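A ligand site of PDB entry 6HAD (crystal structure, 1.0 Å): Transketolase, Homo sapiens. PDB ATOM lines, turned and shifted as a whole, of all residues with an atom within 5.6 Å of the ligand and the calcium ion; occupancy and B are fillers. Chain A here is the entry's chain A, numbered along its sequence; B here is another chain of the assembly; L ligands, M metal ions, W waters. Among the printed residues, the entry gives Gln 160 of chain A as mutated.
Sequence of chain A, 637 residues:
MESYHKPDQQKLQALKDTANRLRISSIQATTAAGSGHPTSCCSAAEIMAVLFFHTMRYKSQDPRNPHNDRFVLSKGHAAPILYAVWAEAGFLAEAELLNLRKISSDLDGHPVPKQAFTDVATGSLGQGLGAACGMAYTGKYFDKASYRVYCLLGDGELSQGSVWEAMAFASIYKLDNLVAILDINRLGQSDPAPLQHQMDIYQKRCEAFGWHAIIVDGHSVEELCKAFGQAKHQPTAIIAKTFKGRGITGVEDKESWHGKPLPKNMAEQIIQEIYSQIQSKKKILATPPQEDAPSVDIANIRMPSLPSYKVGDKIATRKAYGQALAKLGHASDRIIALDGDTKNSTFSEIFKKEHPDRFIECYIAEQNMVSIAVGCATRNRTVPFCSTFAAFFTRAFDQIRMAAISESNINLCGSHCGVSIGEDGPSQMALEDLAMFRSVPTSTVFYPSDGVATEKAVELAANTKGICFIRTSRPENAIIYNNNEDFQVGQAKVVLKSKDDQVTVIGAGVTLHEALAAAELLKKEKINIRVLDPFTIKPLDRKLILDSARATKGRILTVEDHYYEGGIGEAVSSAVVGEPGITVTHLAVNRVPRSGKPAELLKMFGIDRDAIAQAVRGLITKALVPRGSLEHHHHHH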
ATOM      1  N   HIS A  37     -14.926  11.169 -18.792  1.00  0.00           N
ATOM      2  CA  HIS A  37     -14.006  11.054 -19.908  1.00  0.00           C
ATOM      3  C   HIS A  37     -14.018   9.633 -20.497  1.00  0.00           C
ATOM      4  O   HIS A  37     -12.978   8.971 -20.527  1.00  0.00           O
ATOM      5  CB  HIS A  37     -12.587  11.421 -19.450  1.00  0.00           C
ATOM      6  CG  HIS A  37     -12.462  12.811 -18.939  1.00  0.00           C
ATOM      7  ND1 HIS A  37     -12.971  13.191 -17.720  1.00  0.00           N
ATOM      8  CD2 HIS A  37     -11.832  13.883 -19.458  1.00  0.00           C
ATOM      9  CE1 HIS A  37     -12.694  14.470 -17.538  1.00  0.00           C
ATOM     10  NE2 HIS A  37     -12.016  14.919 -18.575  1.00  0.00           N
ATOM     11  N   SER A  40     -11.232   8.677 -22.990  1.00  0.00           N
ATOM     12  CA  SER A  40      -9.903   8.505 -22.391  1.00  0.00           C
ATOM     13  C   SER A  40      -9.806   7.165 -21.671  1.00  0.00           C
ATOM     14  O   SER A  40      -8.718   6.613 -21.506  1.00  0.00           O
ATOM     15  CB  SER A  40      -9.654   9.617 -21.394  1.00  0.00           C
ATOM     16  OG  SER A  40      -9.710  10.899 -21.985  1.00  0.00           O
ATOM     17  N   SER A  43      -9.422   4.145 -24.705  1.00  0.00           N
ATOM     18  CA  SER A  43      -8.118   3.902 -25.314  1.00  0.00           C
ATOM     19  C   SER A  43      -7.271   2.982 -24.455  1.00  0.00           C
ATOM     20  O   SER A  43      -6.370   2.328 -24.973  1.00  0.00           O
ATOM     21  CB  SER A  43      -7.332   5.173 -25.644  1.00  0.00           C
ATOM     22  OG  SER A  43      -7.178   6.018 -24.517  1.00  0.00           O
ATOM     23  N   LYS A  75      -2.774   9.509 -15.821  1.00  0.00           N
ATOM     24  CA  LYS A  75      -3.836  10.188 -16.571  1.00  0.00           C
ATOM     25  C   LYS A  75      -5.125  10.006 -15.779  1.00  0.00           C
ATOM     26  O   LYS A  75      -5.996   9.201 -16.092  1.00  0.00           O
ATOM     27  CB  LYS A  75      -3.922   9.699 -18.032  1.00  0.00           C
ATOM     28  CG  LYS A  75      -3.808   8.201 -18.284  1.00  0.00           C
ATOM     29  CD  LYS A  75      -4.147   7.846 -19.721  1.00  0.00           C
ATOM     30  CE  LYS A  75      -5.627   7.614 -19.914  1.00  0.00           C
ATOM     31  NZ  LYS A  75      -6.005   7.472 -21.320  1.00  0.00           N
ATOM     32  N   HIS A  77      -7.893  11.453 -15.166  1.00  0.00           N
ATOM     33  CA  HIS A  77      -9.251  11.656 -15.666  1.00  0.00           C
ATOM     34  C   HIS A  77      -9.817  10.354 -16.259  1.00  0.00           C
ATOM     35  O   HIS A  77     -11.017  10.279 -16.539  1.00  0.00           O
ATOM     36  CB  HIS A  77      -9.279  12.801 -16.684  1.00  0.00           C
ATOM     37  CG  HIS A  77      -8.285  12.638 -17.773  1.00  0.00           C
ATOM     38  ND1 HIS A  77      -6.915  12.780 -17.588  1.00  0.00           N
ATOM     39  CD2 HIS A  77      -8.468  12.281 -19.058  1.00  0.00           C
ATOM     40  CE1 HIS A  77      -6.322  12.542 -18.744  1.00  0.00           C
ATOM     41  NE2 HIS A  77      -7.243  12.233 -19.646  1.00  0.00           N
ATOM     42  N   GLY A 123      -4.618  13.918 -11.353  1.00  0.00           N
ATOM     43  CA  GLY A 123      -5.530  14.846 -11.932  1.00  0.00           C
ATOM     44  C   GLY A 123      -4.776  16.050 -12.454  1.00  0.00           C
ATOM     45  O   GLY A 123      -5.217  16.641 -13.413  1.00  0.00           O
ATOM     46  N   SER A 124      -3.663  16.408 -11.817  1.00  0.00           N
ATOM     47  CA  SER A 124      -2.735  17.349 -12.406  1.00  0.00           C
ATOM     48  C   SER A 124      -1.755  16.508 -13.209  1.00  0.00           C
ATOM     49  O   SER A 124      -0.962  15.739 -12.647  1.00  0.00           O
ATOM     50  CB  SER A 124      -2.011  18.166 -11.367  1.00  0.00           C
ATOM     51  OG  SER A 124      -0.996  18.861 -12.059  1.00  0.00           O
ATOM     52  N   LEU A 125      -1.821  16.618 -14.518  1.00  0.00           N
ATOM     53  CA  LEU A 125      -1.083  15.721 -15.379  1.00  0.00           C
ATOM     54  C   LEU A 125       0.424  15.843 -15.223  1.00  0.00           C
ATOM     55  O   LEU A 125       0.959  16.907 -14.968  1.00  0.00           O
ATOM     56  CB  LEU A 125      -1.468  16.000 -16.833  1.00  0.00           C
ATOM     57  CG  LEU A 125      -2.876  15.558 -17.195  1.00  0.00           C
ATOM     58  CD1 LEU A 125      -3.284  16.169 -18.492  1.00  0.00           C
ATOM     59  CD2 LEU A 125      -2.937  14.036 -17.305  1.00  0.00           C
ATOM     60  N   GLY A 154      -0.916   9.445 -20.309  1.00  0.00           N
ATOM     61  CA  GLY A 154      -1.399   9.884 -21.611  1.00  0.00           C
ATOM     62  C   GLY A 154      -0.301  10.445 -22.485  1.00  0.00           C
ATOM     63  O   GLY A 154       0.805  10.711 -22.020  1.00  0.00           O
ATOM     64  N   ASP A 155      -0.599  10.651 -23.771  1.00  0.00           N
ATOM     65  CA  ASP A 155       0.390  11.228 -24.652  1.00  0.00           C
ATOM     66  C   ASP A 155       0.479  12.746 -24.566  1.00  0.00           C
ATOM     67  O   ASP A 155       1.585  13.277 -24.558  1.00  0.00           O
ATOM     68  CB  ASP A 155       0.301  10.726 -26.119  1.00  0.00           C
ATOM     69  CG  ASP A 155      -1.049  10.907 -26.824  1.00  0.00           C
ATOM     70  OD1 ASP A 155      -2.030  11.346 -26.222  1.00  0.00           O
ATOM     71  OD2 ASP A 155      -1.082  10.561 -28.028  1.00  0.00           O
ATOM     72  N   GLY A 156      -0.648  13.444 -24.446  1.00  0.00           N
ATOM     73  CA  GLY A 156      -0.599  14.869 -24.166  1.00  0.00           C
ATOM     74  C   GLY A 156       0.217  15.150 -22.907  1.00  0.00           C
ATOM     75  O   GLY A 156       1.011  16.096 -22.825  1.00  0.00           O
ATOM     76  N   GLU A 157       0.005  14.313 -21.914  1.00  0.00           N
ATOM     77  CA  GLU A 157       0.670  14.372 -20.650  1.00  0.00           C
ATOM     78  C   GLU A 157       2.203  14.393 -20.781  1.00  0.00           C
ATOM     79  O   GLU A 157       2.891  14.995 -19.946  1.00  0.00           O
ATOM     80  CB  GLU A 157       0.222  13.159 -19.808  1.00  0.00           C
ATOM     81  CG  GLU A 157       0.846  13.095 -18.470  1.00  0.00           C
ATOM     82  CD  GLU A 157       0.176  12.083 -17.525  1.00  0.00           C
ATOM     83  OE1 GLU A 157      -0.420  11.059 -17.978  1.00  0.00           O
ATOM     84  OE2 GLU A 157       0.297  12.288 -16.311  1.00  0.00           O
ATOM     85  N   LEU A 158       2.747  13.748 -21.808  1.00  0.00           N
ATOM     86  CA  LEU A 158       4.185  13.665 -22.039  1.00  0.00           C
ATOM     87  C   LEU A 158       4.812  15.001 -22.419  1.00  0.00           C
ATOM     88  O   LEU A 158       6.027  15.098 -22.490  1.00  0.00           O
ATOM     89  CB  LEU A 158       4.508  12.602 -23.086  1.00  0.00           C
ATOM     90  CG  LEU A 158       3.947  11.230 -22.766  1.00  0.00           C
ATOM     91  CD1 LEU A 158       4.166  10.293 -23.949  1.00  0.00           C
ATOM     92  CD2 LEU A 158       4.519  10.662 -21.476  1.00  0.00           C
ATOM     93  N   GLN A 160       4.688  17.416 -20.344  1.00  0.00           N
ATOM     94  CA  GLN A 160       5.125  17.956 -19.053  1.00  0.00           C
ATOM     95  C   GLN A 160       6.563  17.605 -18.755  1.00  0.00           C
ATOM     96  O   GLN A 160       6.964  16.424 -18.764  1.00  0.00           O
ATOM     97  CB  GLN A 160       4.260  17.414 -17.913  1.00  0.00           C
ATOM     98  CG  GLN A 160       2.853  17.974 -17.878  1.00  0.00           C
ATOM     99  CD  GLN A 160       2.789  19.393 -17.362  1.00  0.00           C
ATOM    100  OE1 GLN A 160       3.799  20.095 -17.209  1.00  0.00           O
ATOM    101  NE2 GLN A 160       1.589  19.825 -17.043  1.00  0.00           N
ATOM    102  N   ASP A 183      -0.144   5.719 -23.275  1.00  0.00           N
ATOM    103  CA  ASP A 183      -1.371   5.573 -24.053  1.00  0.00           C
ATOM    104  C   ASP A 183      -1.313   6.575 -25.188  1.00  0.00           C
ATOM    105  O   ASP A 183      -1.778   7.708 -25.065  1.00  0.00           O
ATOM    106  CB  ASP A 183      -2.566   5.772 -23.115  1.00  0.00           C
ATOM    107  CG  ASP A 183      -3.916   5.553 -23.779  1.00  0.00           C
ATOM    108  OD1 ASP A 183      -3.967   5.344 -25.005  1.00  0.00           O
ATOM    109  OD2 ASP A 183      -4.943   5.627 -23.051  1.00  0.00           O
ATOM    110  N   ASN A 185      -2.778   7.755 -27.868  1.00  0.00           N
ATOM    111  CA  ASN A 185      -4.061   7.758 -28.559  1.00  0.00           C
ATOM    112  C   ASN A 185      -4.245   8.953 -29.483  1.00  0.00           C
ATOM    113  O   ASN A 185      -5.373   9.192 -29.959  1.00  0.00           O
ATOM    114  CB  ASN A 185      -5.228   7.602 -27.585  1.00  0.00           C
ATOM    115  CG  ASN A 185      -5.412   8.790 -26.683  1.00  0.00           C
ATOM    116  OD1 ASN A 185      -4.873   9.866 -26.934  1.00  0.00           O
ATOM    117  ND2 ASN A 185      -6.167   8.595 -25.616  1.00  0.00           N
ATOM    118  N   ARG A 186      -3.170   9.656 -29.775  1.00  0.00           N
ATOM    119  CA  ARG A 186      -3.071  10.668 -30.836  1.00  0.00           C
ATOM    120  C   ARG A 186      -3.584  12.043 -30.441  1.00  0.00           C
ATOM    121  O   ARG A 186      -3.106  13.026 -30.980  1.00  0.00           O
ATOM    122  CB  ARG A 186      -3.738  10.216 -32.137  1.00  0.00           C
ATOM    123  CG  ARG A 186      -3.228  10.960 -33.358  1.00  0.00           C
ATOM    124  CD  ARG A 186      -3.912  10.485 -34.636  1.00  0.00           C
ATOM    125  NE  ARG A 186      -5.365  10.697 -34.661  1.00  0.00           N
ATOM    126  CZ  ARG A 186      -5.968  11.829 -34.990  1.00  0.00           C
ATOM    127  NH1 ARG A 186      -7.296  11.888 -35.014  1.00  0.00           N
ATOM    128  NH2 ARG A 186      -5.238  12.896 -35.289  1.00  0.00           N
ATOM    129  N   LEU A 187      -4.580  12.089 -29.557  1.00  0.00           N
ATOM    130  CA  LEU A 187      -5.329  13.290 -29.277  1.00  0.00           C
ATOM    131  C   LEU A 187      -5.153  13.765 -27.850  1.00  0.00           C
ATOM    132  O   LEU A 187      -5.123  12.964 -26.926  1.00  0.00           O
ATOM    133  CB  LEU A 187      -6.817  13.071 -29.541  1.00  0.00           C
ATOM    134  CG  LEU A 187      -7.189  12.723 -30.977  1.00  0.00           C
ATOM    135  CD1 LEU A 187      -8.690  12.483 -31.075  1.00  0.00           C
ATOM    136  CD2 LEU A 187      -6.724  13.780 -31.938  1.00  0.00           C
ATOM    137  N   GLY A 188      -5.111  15.079 -27.668  1.00  0.00           N
ATOM    138  CA  GLY A 188      -5.178  15.687 -26.354  1.00  0.00           C
ATOM    139  C   GLY A 188      -6.598  16.159 -26.085  1.00  0.00           C
ATOM    140  O   GLY A 188      -7.567  15.521 -26.522  1.00  0.00           O
ATOM    141  N   GLN A 189      -6.727  17.262 -25.352  1.00  0.00           N
ATOM    142  CA  GLN A 189      -8.032  17.800 -24.997  1.00  0.00           C
ATOM    143  C   GLN A 189      -8.656  18.616 -26.121  1.00  0.00           C
ATOM    144  O   GLN A 189      -9.855  18.515 -26.364  1.00  0.00           O
ATOM    145  CB  GLN A 189      -7.902  18.661 -23.741  1.00  0.00           C
ATOM    146  CG  GLN A 189      -9.150  19.497 -23.480  1.00  0.00           C
ATOM    147  CD  GLN A 189      -9.221  20.102 -22.108  1.00  0.00           C
ATOM    148  OE1 GLN A 189      -8.739  19.529 -21.124  1.00  0.00           O
ATOM    149  NE2 GLN A 189      -9.821  21.276 -22.014  1.00  0.00           N
ATOM    150  N   ALA A 193      -2.273  15.589 -29.984  1.00  0.00           N
ATOM    151  CA  ALA A 193      -1.021  15.729 -29.271  1.00  0.00           C
ATOM    152  C   ALA A 193       0.089  16.015 -30.299  1.00  0.00           C
ATOM    153  O   ALA A 193      -0.010  15.572 -31.435  1.00  0.00           O
ATOM    154  CB  ALA A 193      -0.716  14.472 -28.465  1.00  0.00           C
ATOM    155  N   LYS A 244      -8.280   6.979 -29.375  1.00  0.00           N
ATOM    156  CA  LYS A 244      -9.120   7.575 -28.360  1.00  0.00           C
ATOM    157  C   LYS A 244     -10.564   7.186 -28.644  1.00  0.00           C
ATOM    158  O   LYS A 244     -10.984   7.158 -29.785  1.00  0.00           O
ATOM    159  CB  LYS A 244      -8.888   9.080 -28.304  1.00  0.00           C
ATOM    160  CG  LYS A 244      -9.318   9.731 -26.987  1.00  0.00           C
ATOM    161  CD  LYS A 244      -8.699  11.110 -26.808  1.00  0.00           C
ATOM    162  CE  LYS A 244      -9.094  11.793 -25.525  1.00  0.00           C
ATOM    163  NZ  LYS A 244      -8.190  12.923 -25.186  1.00  0.00           N
ATOM    164  N   HIS A 258     -13.154  14.872 -26.021  1.00  0.00           N
ATOM    165  CA  HIS A 258     -12.428  14.786 -24.774  1.00  0.00           C
ATOM    166  C   HIS A 258     -13.322  15.295 -23.636  1.00  0.00           C
ATOM    167  O   HIS A 258     -13.836  16.412 -23.686  1.00  0.00           O
ATOM    168  CB  HIS A 258     -11.147  15.599 -24.789  1.00  0.00           C
ATOM    169  CG  HIS A 258     -10.397  15.506 -23.508  1.00  0.00           C
ATOM    170  ND1 HIS A 258      -9.503  14.493 -23.242  1.00  0.00           N
ATOM    171  CD2 HIS A 258     -10.443  16.285 -22.405  1.00  0.00           C
ATOM    172  CE1 HIS A 258      -9.040  14.665 -22.022  1.00  0.00           C
ATOM    173  NE2 HIS A 258      -9.591  15.741 -21.492  1.00  0.00           N
ATOM    174  N   ASP A 398       2.759  22.770  -7.550  1.00  0.00           N
ATOM    175  CA  ASP A 398       1.653  21.885  -7.939  1.00  0.00           C
ATOM    176  C   ASP A 398       1.822  20.477  -7.348  1.00  0.00           C
ATOM    177  O   ASP A 398       0.865  19.823  -6.968  1.00  0.00           O
ATOM    178  CB  ASP A 398       1.547  21.874  -9.459  1.00  0.00           C
ATOM    179  CG  ASP A 398       0.256  21.260 -10.023  1.00  0.00           C
ATOM    180  OD1 ASP A 398      -0.757  21.166  -9.306  1.00  0.00           O
ATOM    181  OD2 ASP A 398       0.308  20.896 -11.218  1.00  0.00           O
ATOM    182  N   GLY B 340      -2.505  26.180 -22.779  1.00  0.00           N
ATOM    183  CA  GLY B 340      -1.905  24.865 -22.601  1.00  0.00           C
ATOM    184  C   GLY B 340      -2.893  23.725 -22.812  1.00  0.00           C
ATOM    185  O   GLY B 340      -3.224  23.028 -21.862  1.00  0.00           O
ATOM    186  N   ASP B 341      -3.348  23.542 -24.047  1.00  0.00           N
ATOM    187  CA  ASP B 341      -4.309  22.484 -24.421  1.00  0.00           C
ATOM    188  C   ASP B 341      -5.629  22.588 -23.653  1.00  0.00           C
ATOM    189  O   ASP B 341      -6.286  21.587 -23.477  1.00  0.00           O
ATOM    190  CB  ASP B 341      -3.727  21.076 -24.307  1.00  0.00           C
ATOM    191  CG  ASP B 341      -4.560  20.009 -25.009  1.00  0.00           C
ATOM    192  OD1 ASP B 341      -5.246  20.322 -26.033  1.00  0.00           O
ATOM    193  OD2 ASP B 341      -4.500  18.835 -24.575  1.00  0.00           O
ATOM    194  N   THR B 342      -5.995  23.802 -23.251  1.00  0.00           N
ATOM    195  CA  THR B 342      -7.254  24.039 -22.539  1.00  0.00           C
ATOM    196  C   THR B 342      -8.124  25.090 -23.192  1.00  0.00           C
ATOM    197  O   THR B 342      -9.057  25.583 -22.576  1.00  0.00           O
ATOM    198  CB  THR B 342      -7.039  24.348 -21.025  1.00  0.00           C
ATOM    199  OG1 THR B 342      -6.128  25.438 -20.820  1.00  0.00           O
ATOM    200  CG2 THR B 342      -6.467  23.142 -20.312  1.00  0.00           C
ATOM    201  N   ILE B 364       0.573  20.786 -23.001  1.00  0.00           N
ATOM    202  CA  ILE B 364       0.381  20.576 -21.553  1.00  0.00           C
ATOM    203  C   ILE B 364       1.744  20.750 -20.900  1.00  0.00           C
ATOM    204  O   ILE B 364       2.457  19.794 -20.590  1.00  0.00           O
ATOM    205  CB  ILE B 364      -0.283  19.225 -21.254  1.00  0.00           C
ATOM    206  CG1 ILE B 364      -1.575  19.058 -22.054  1.00  0.00           C
ATOM    207  CG2 ILE B 364      -0.520  19.070 -19.778  1.00  0.00           C
ATOM    208  CD1 ILE B 364      -2.232  17.675 -21.925  1.00  0.00           C
ATOM    209  N   GLU B 366       2.771  24.051 -18.595  1.00  0.00           N
ATOM    210  CA  GLU B 366       2.498  25.387 -18.080  1.00  0.00           C
ATOM    211  C   GLU B 366       3.753  26.177 -17.723  1.00  0.00           C
ATOM    212  O   GLU B 366       3.765  27.387 -17.874  1.00  0.00           O
ATOM    213  CB  GLU B 366       1.563  25.335 -16.881  1.00  0.00           C
ATOM    214  CG  GLU B 366       0.178  24.761 -17.165  1.00  0.00           C
ATOM    215  CD  GLU B 366       0.099  23.242 -17.174  1.00  0.00           C
ATOM    216  OE1 GLU B 366       1.049  22.567 -16.736  1.00  0.00           O
ATOM    217  OE2 GLU B 366      -0.958  22.745 -17.621  1.00  0.00           O
ATOM    218  N   THR B 388      -4.948  28.991 -18.712  1.00  0.00           N
ATOM    219  CA  THR B 388      -5.161  27.599 -18.351  1.00  0.00           C
ATOM    220  C   THR B 388      -6.133  27.601 -17.174  1.00  0.00           C
ATOM    221  O   THR B 388      -6.676  28.644 -16.813  1.00  0.00           O
ATOM    222  CB  THR B 388      -3.817  26.860 -18.035  1.00  0.00           C
ATOM    223  OG1 THR B 388      -4.104  25.506 -17.664  1.00  0.00           O
ATOM    224  CG2 THR B 388      -3.068  27.471 -16.871  1.00  0.00           C
ATOM    225  N   PHE B 389      -6.383  26.451 -16.563  1.00  0.00           N
ATOM    226  CA  PHE B 389      -7.089  26.426 -15.290  1.00  0.00           C
ATOM    227  C   PHE B 389      -6.204  27.083 -14.223  1.00  0.00           C
ATOM    228  O   PHE B 389      -5.003  26.824 -14.170  1.00  0.00           O
ATOM    229  CB  PHE B 389      -7.358  24.993 -14.815  1.00  0.00           C
ATOM    230  CG  PHE B 389      -8.407  24.246 -15.580  1.00  0.00           C
ATOM    231  CD1 PHE B 389      -8.665  24.478 -16.891  1.00  0.00           C
ATOM    232  CD2 PHE B 389      -9.150  23.291 -14.911  1.00  0.00           C
ATOM    233  CE1 PHE B 389      -9.647  23.734 -17.547  1.00  0.00           C
ATOM    234  CE2 PHE B 389     -10.114  22.544 -15.540  1.00  0.00           C
ATOM    235  CZ  PHE B 389     -10.363  22.765 -16.865  1.00  0.00           C
ATOM    236  N   PHE B 392      -3.592  25.090 -12.324  1.00  0.00           N
ATOM    237  CA  PHE B 392      -2.366  24.672 -12.980  1.00  0.00           C
ATOM    238  C   PHE B 392      -1.347  25.772 -13.117  1.00  0.00           C
ATOM    239  O   PHE B 392      -0.188  25.474 -13.456  1.00  0.00           O
ATOM    240  CB  PHE B 392      -2.650  23.928 -14.297  1.00  0.00           C
ATOM    241  CG  PHE B 392      -3.626  22.800 -14.126  1.00  0.00           C
ATOM    242  CD1 PHE B 392      -3.539  21.946 -13.025  1.00  0.00           C
ATOM    243  CD2 PHE B 392      -4.674  22.634 -15.007  1.00  0.00           C
ATOM    244  CE1 PHE B 392      -4.460  20.925 -12.837  1.00  0.00           C
ATOM    245  CE2 PHE B 392      -5.608  21.629 -14.812  1.00  0.00           C
ATOM    246  CZ  PHE B 392      -5.488  20.797 -13.722  1.00  0.00           C
ATOM    247  N   ARG B 395       1.748  25.072 -11.123  1.00  0.00           N
ATOM    248  CA  ARG B 395       2.822  24.326 -11.790  1.00  0.00           C
ATOM    249  C   ARG B 395       3.921  25.269 -12.305  1.00  0.00           C
ATOM    250  O   ARG B 395       5.032  24.805 -12.595  1.00  0.00           O
ATOM    251  CB  ARG B 395       2.201  23.516 -12.929  1.00  0.00           C
ATOM    252  CG  ARG B 395       3.113  22.472 -13.579  1.00  0.00           C
ATOM    253  CD  ARG B 395       3.608  21.434 -12.595  1.00  0.00           C
ATOM    254  NE  ARG B 395       3.950  20.208 -13.271  1.00  0.00           N
ATOM    255  CZ  ARG B 395       3.035  19.287 -13.586  1.00  0.00           C
ATOM    256  NH1 ARG B 395       1.753  19.463 -13.280  1.00  0.00           N
ATOM    257  NH2 ARG B 395       3.393  18.209 -14.259  1.00  0.00           N
ATOM    258  N   GLN B 428      -8.572  19.848  -9.876  1.00  0.00           N
ATOM    259  CA  GLN B 428      -8.834  20.896 -10.870  1.00  0.00           C
ATOM    260  C   GLN B 428      -9.244  22.222 -10.232  1.00  0.00           C
ATOM    261  O   GLN B 428      -9.446  23.181 -10.962  1.00  0.00           O
ATOM    262  CB  GLN B 428      -9.953  20.437 -11.841  1.00  0.00           C
ATOM    263  CG  GLN B 428      -9.839  18.949 -12.342  1.00  0.00           C
ATOM    264  CD  GLN B 428      -8.585  18.632 -13.120  1.00  0.00           C
ATOM    265  OE1 GLN B 428      -7.742  17.821 -12.680  1.00  0.00           O
ATOM    266  NE2 GLN B 428      -8.419  19.275 -14.254  1.00  0.00           N
HETATM  267  N1  LIG L   1      -2.650  20.771 -17.068  1.00  0.00           N
HETATM  268  C1  LIG L   1      -2.444  19.921 -16.068  1.00  0.00           C
HETATM  269  C2  LIG L   1      -1.174  20.049 -15.292  1.00  0.00           C
HETATM  270  N2  LIG L   1      -3.336  18.992 -15.738  1.00  0.00           N
HETATM  271  C3  LIG L   1      -4.496  18.926 -16.384  1.00  0.00           C
HETATM  272  N3  LIG L   1      -5.368  18.035 -15.944  1.00  0.00           N
HETATM  273  C4  LIG L   1      -4.775  19.806 -17.522  1.00  0.00           C
HETATM  274  C5  LIG L   1      -3.770  20.722 -17.802  1.00  0.00           C
HETATM  275  C6  LIG L   1      -6.123  19.798 -18.272  1.00  0.00           C
HETATM  276  N4  LIG L   1      -6.343  18.522 -18.933  1.00  0.00           N
HETATM  277  C7  LIG L   1      -7.065  17.490 -18.431  1.00  0.00           C
HETATM  278  S1  LIG L   1      -7.070  16.056 -19.375  1.00  0.00           S
HETATM  279  C8  LIG L   1      -6.161  16.942 -20.598  1.00  0.00           C
HETATM  280  C9  LIG L   1      -5.886  18.286 -20.186  1.00  0.00           C
HETATM  281  C10 LIG L   1      -5.133  19.269 -21.000  1.00  0.00           C
HETATM  282  C11 LIG L   1      -5.780  16.293 -21.861  1.00  0.00           C
HETATM  283  C12 LIG L   1      -4.982  15.052 -21.524  1.00  0.00           C
HETATM  284  O1  LIG L   1      -4.630  14.415 -22.729  1.00  0.00           O
HETATM  285  P1  LIG L   1      -3.751  13.084 -22.698  1.00  0.00           P
HETATM  286  O2  LIG L   1      -2.631  13.182 -21.732  1.00  0.00           O
HETATM  287  O3  LIG L   1      -3.407  12.860 -24.114  1.00  0.00           O
HETATM  288  O4  LIG L   1      -4.792  11.975 -22.168  1.00  0.00           O
HETATM  289  P2  LIG L   1      -5.984  11.165 -22.912  1.00  0.00           P
HETATM  290  O5  LIG L   1      -5.916  11.462 -24.392  1.00  0.00           O
HETATM  291  O6  LIG L   1      -5.666   9.728 -22.635  1.00  0.00           O
HETATM  292  O7  LIG L   1      -7.239  11.690 -22.261  1.00  0.00           O
HETATM  293 CA    CA M   1      -4.112  11.488 -25.644  1.00  0.00          CA
HETATM  294  O   HOH W   1     -10.455  17.202 -19.033  1.00  0.00           O
HETATM  295  O   HOH W   2      -2.879  23.686 -19.216  1.00  0.00           O
HETATM  296  O   HOH W   3      -3.470   9.669 -24.264  1.00  0.00           O
HETATM  297  O   HOH W   4      -9.749  19.621 -18.665  1.00  0.00           O
HETATM  298  O   HOH W   5      -7.942  16.170 -15.598  1.00  0.00           O
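A ring nitrogen (NE2) of His 77 is in hydrogen-bond range of an oxygen (O7) of the ligand. N1 of the ligand lies within hydrogen-bond range of OE2 of Glu 366 of chain B, 2.7 Å away. N of Gly 156 sits at hydrogen-bond distance from O2 of the ligand, 3.4 Å away. A ring nitrogen (NE2) of His 258 lies close to a sulfur (S1) of the ligand (3.3 Å). The backbone NH of Leu 125 lies within hydrogen-bond range of a nitrogen (N2) of the ligand, 3.1 Å away. An oxygen (O7) of the ligand is in salt-bridge range of the side-chain amino group (NZ) of Lys 244 (3.3 Å). The backbone NH (N) of Glu 157 sits at hydrogen-bond distance from an oxygen (O2) of the ligand. O of Gly 123 sits at hydrogen-bond distance from N3 of the ligand (2.9 Å). The side-chain amino group of Lys 75 lies within salt-bridge range of an oxygen (O6) of the ligand, at 2.6 Å. The side-chain hydroxyl (OG) of Ser 40 sits at hydrogen-bond distance from an oxygen (O7) of the ligand (2.6 Å).
A ring nitrogen (ND1) of His 258 is in hydrogen-bond range of the side-chain amino group of Lys 244 (2.8 Å). The backbone carbonyl oxygen of Ser 40 lies within hydrogen-bond range of the side-chain hydroxyl of Ser 43 (3.4 Å). The side-chain carboxylate (OE1) of Glu 366 of chain B lies within hydrogen-bond range of the side-chain amide nitrogen (NE2) of Gln 160 (2.8 Å). The backbone NH (N) of Gln 189 lies within hydrogen-bond range of the side-chain carboxylate (OD2) of Asp 341 of chain B (2.8 Å). The backbone NH (N) of Asp 155 is in hydrogen-bond range of the backbone carbonyl oxygen (O) of Asp 183 (3.4 Å). OG of Ser 124 is in hydrogen-bond range of OD2 of Asp 398 (2.6 Å). OD2 of Asp 183 lies within salt-bridge range of NZ of Lys 75. O of Leu 125 sits at hydrogen-bond distance from NH2 of Arg 395 of chain B (2.8 Å).
N4 of the ligand lies close to OE1 of Gln 189 (3.4 Å). Merely in contact with the ligand: Ser 124 (3.4 Å), Gly 154 (3.5 Å), Gln 160 (3.3 Å), Gly 188 (3.9 Å), Asp 341 of chain B (3.6 Å), Thr 342 of chain B (3.9 Å), Ile 364 of chain B (3.4 Å), Phe 392 of chain B (3.3 Å), Arg 395 of chain B (3.6 Å) and Gln 428 of chain B (3.7 Å). Hydrophobic or aromatic side chains that line the ligand: His 77, Leu 125, His 258, Ile 364 of chain B and Phe 392 of chain B.
The nearest printed residue that does not touch the calcium ion is Gly 156 (4.2 Å).
OD1 of Asp 155 is bound to the calcium ion. The calcium ion is bound by O3 of the ligand, at 2.2 Å. An oxygen (O5) of the ligand is bound to the calcium ion (2.2 Å). The backbone carbonyl oxygen (O) of Leu 187 binds the calcium ion, at 2.2 Å. The side-chain amide oxygen (OD1) of Asn 185 binds the calcium ion (2.2 Å). Water W3 is bound to the calcium ion. The calcium ion has six donor atoms within binding distance.
Water W3 lies within hydrogen-bond range of O of Asp 183, O6 of the ligand, N of Asp 155 and ND2 of Asn 185. Water W5 lies within hydrogen-bond range of a nitrogen (N3) of the ligand (3.2 Å) and the side-chain amide oxygen of Gln 428 of chain B (3.4 Å). Water W2 lies within hydrogen-bond range of the side-chain carboxylate of Glu 366 of chain B (2.7 Å) and the backbone carbonyl oxygen of Gly 340 of chain B (2.7 Å). Water W1 lies within hydrogen-bond range of NE2 of His 37 (2.8 Å), NE2 of His 258 (3.0 Å) and S1 of the ligand (3.6 Å).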
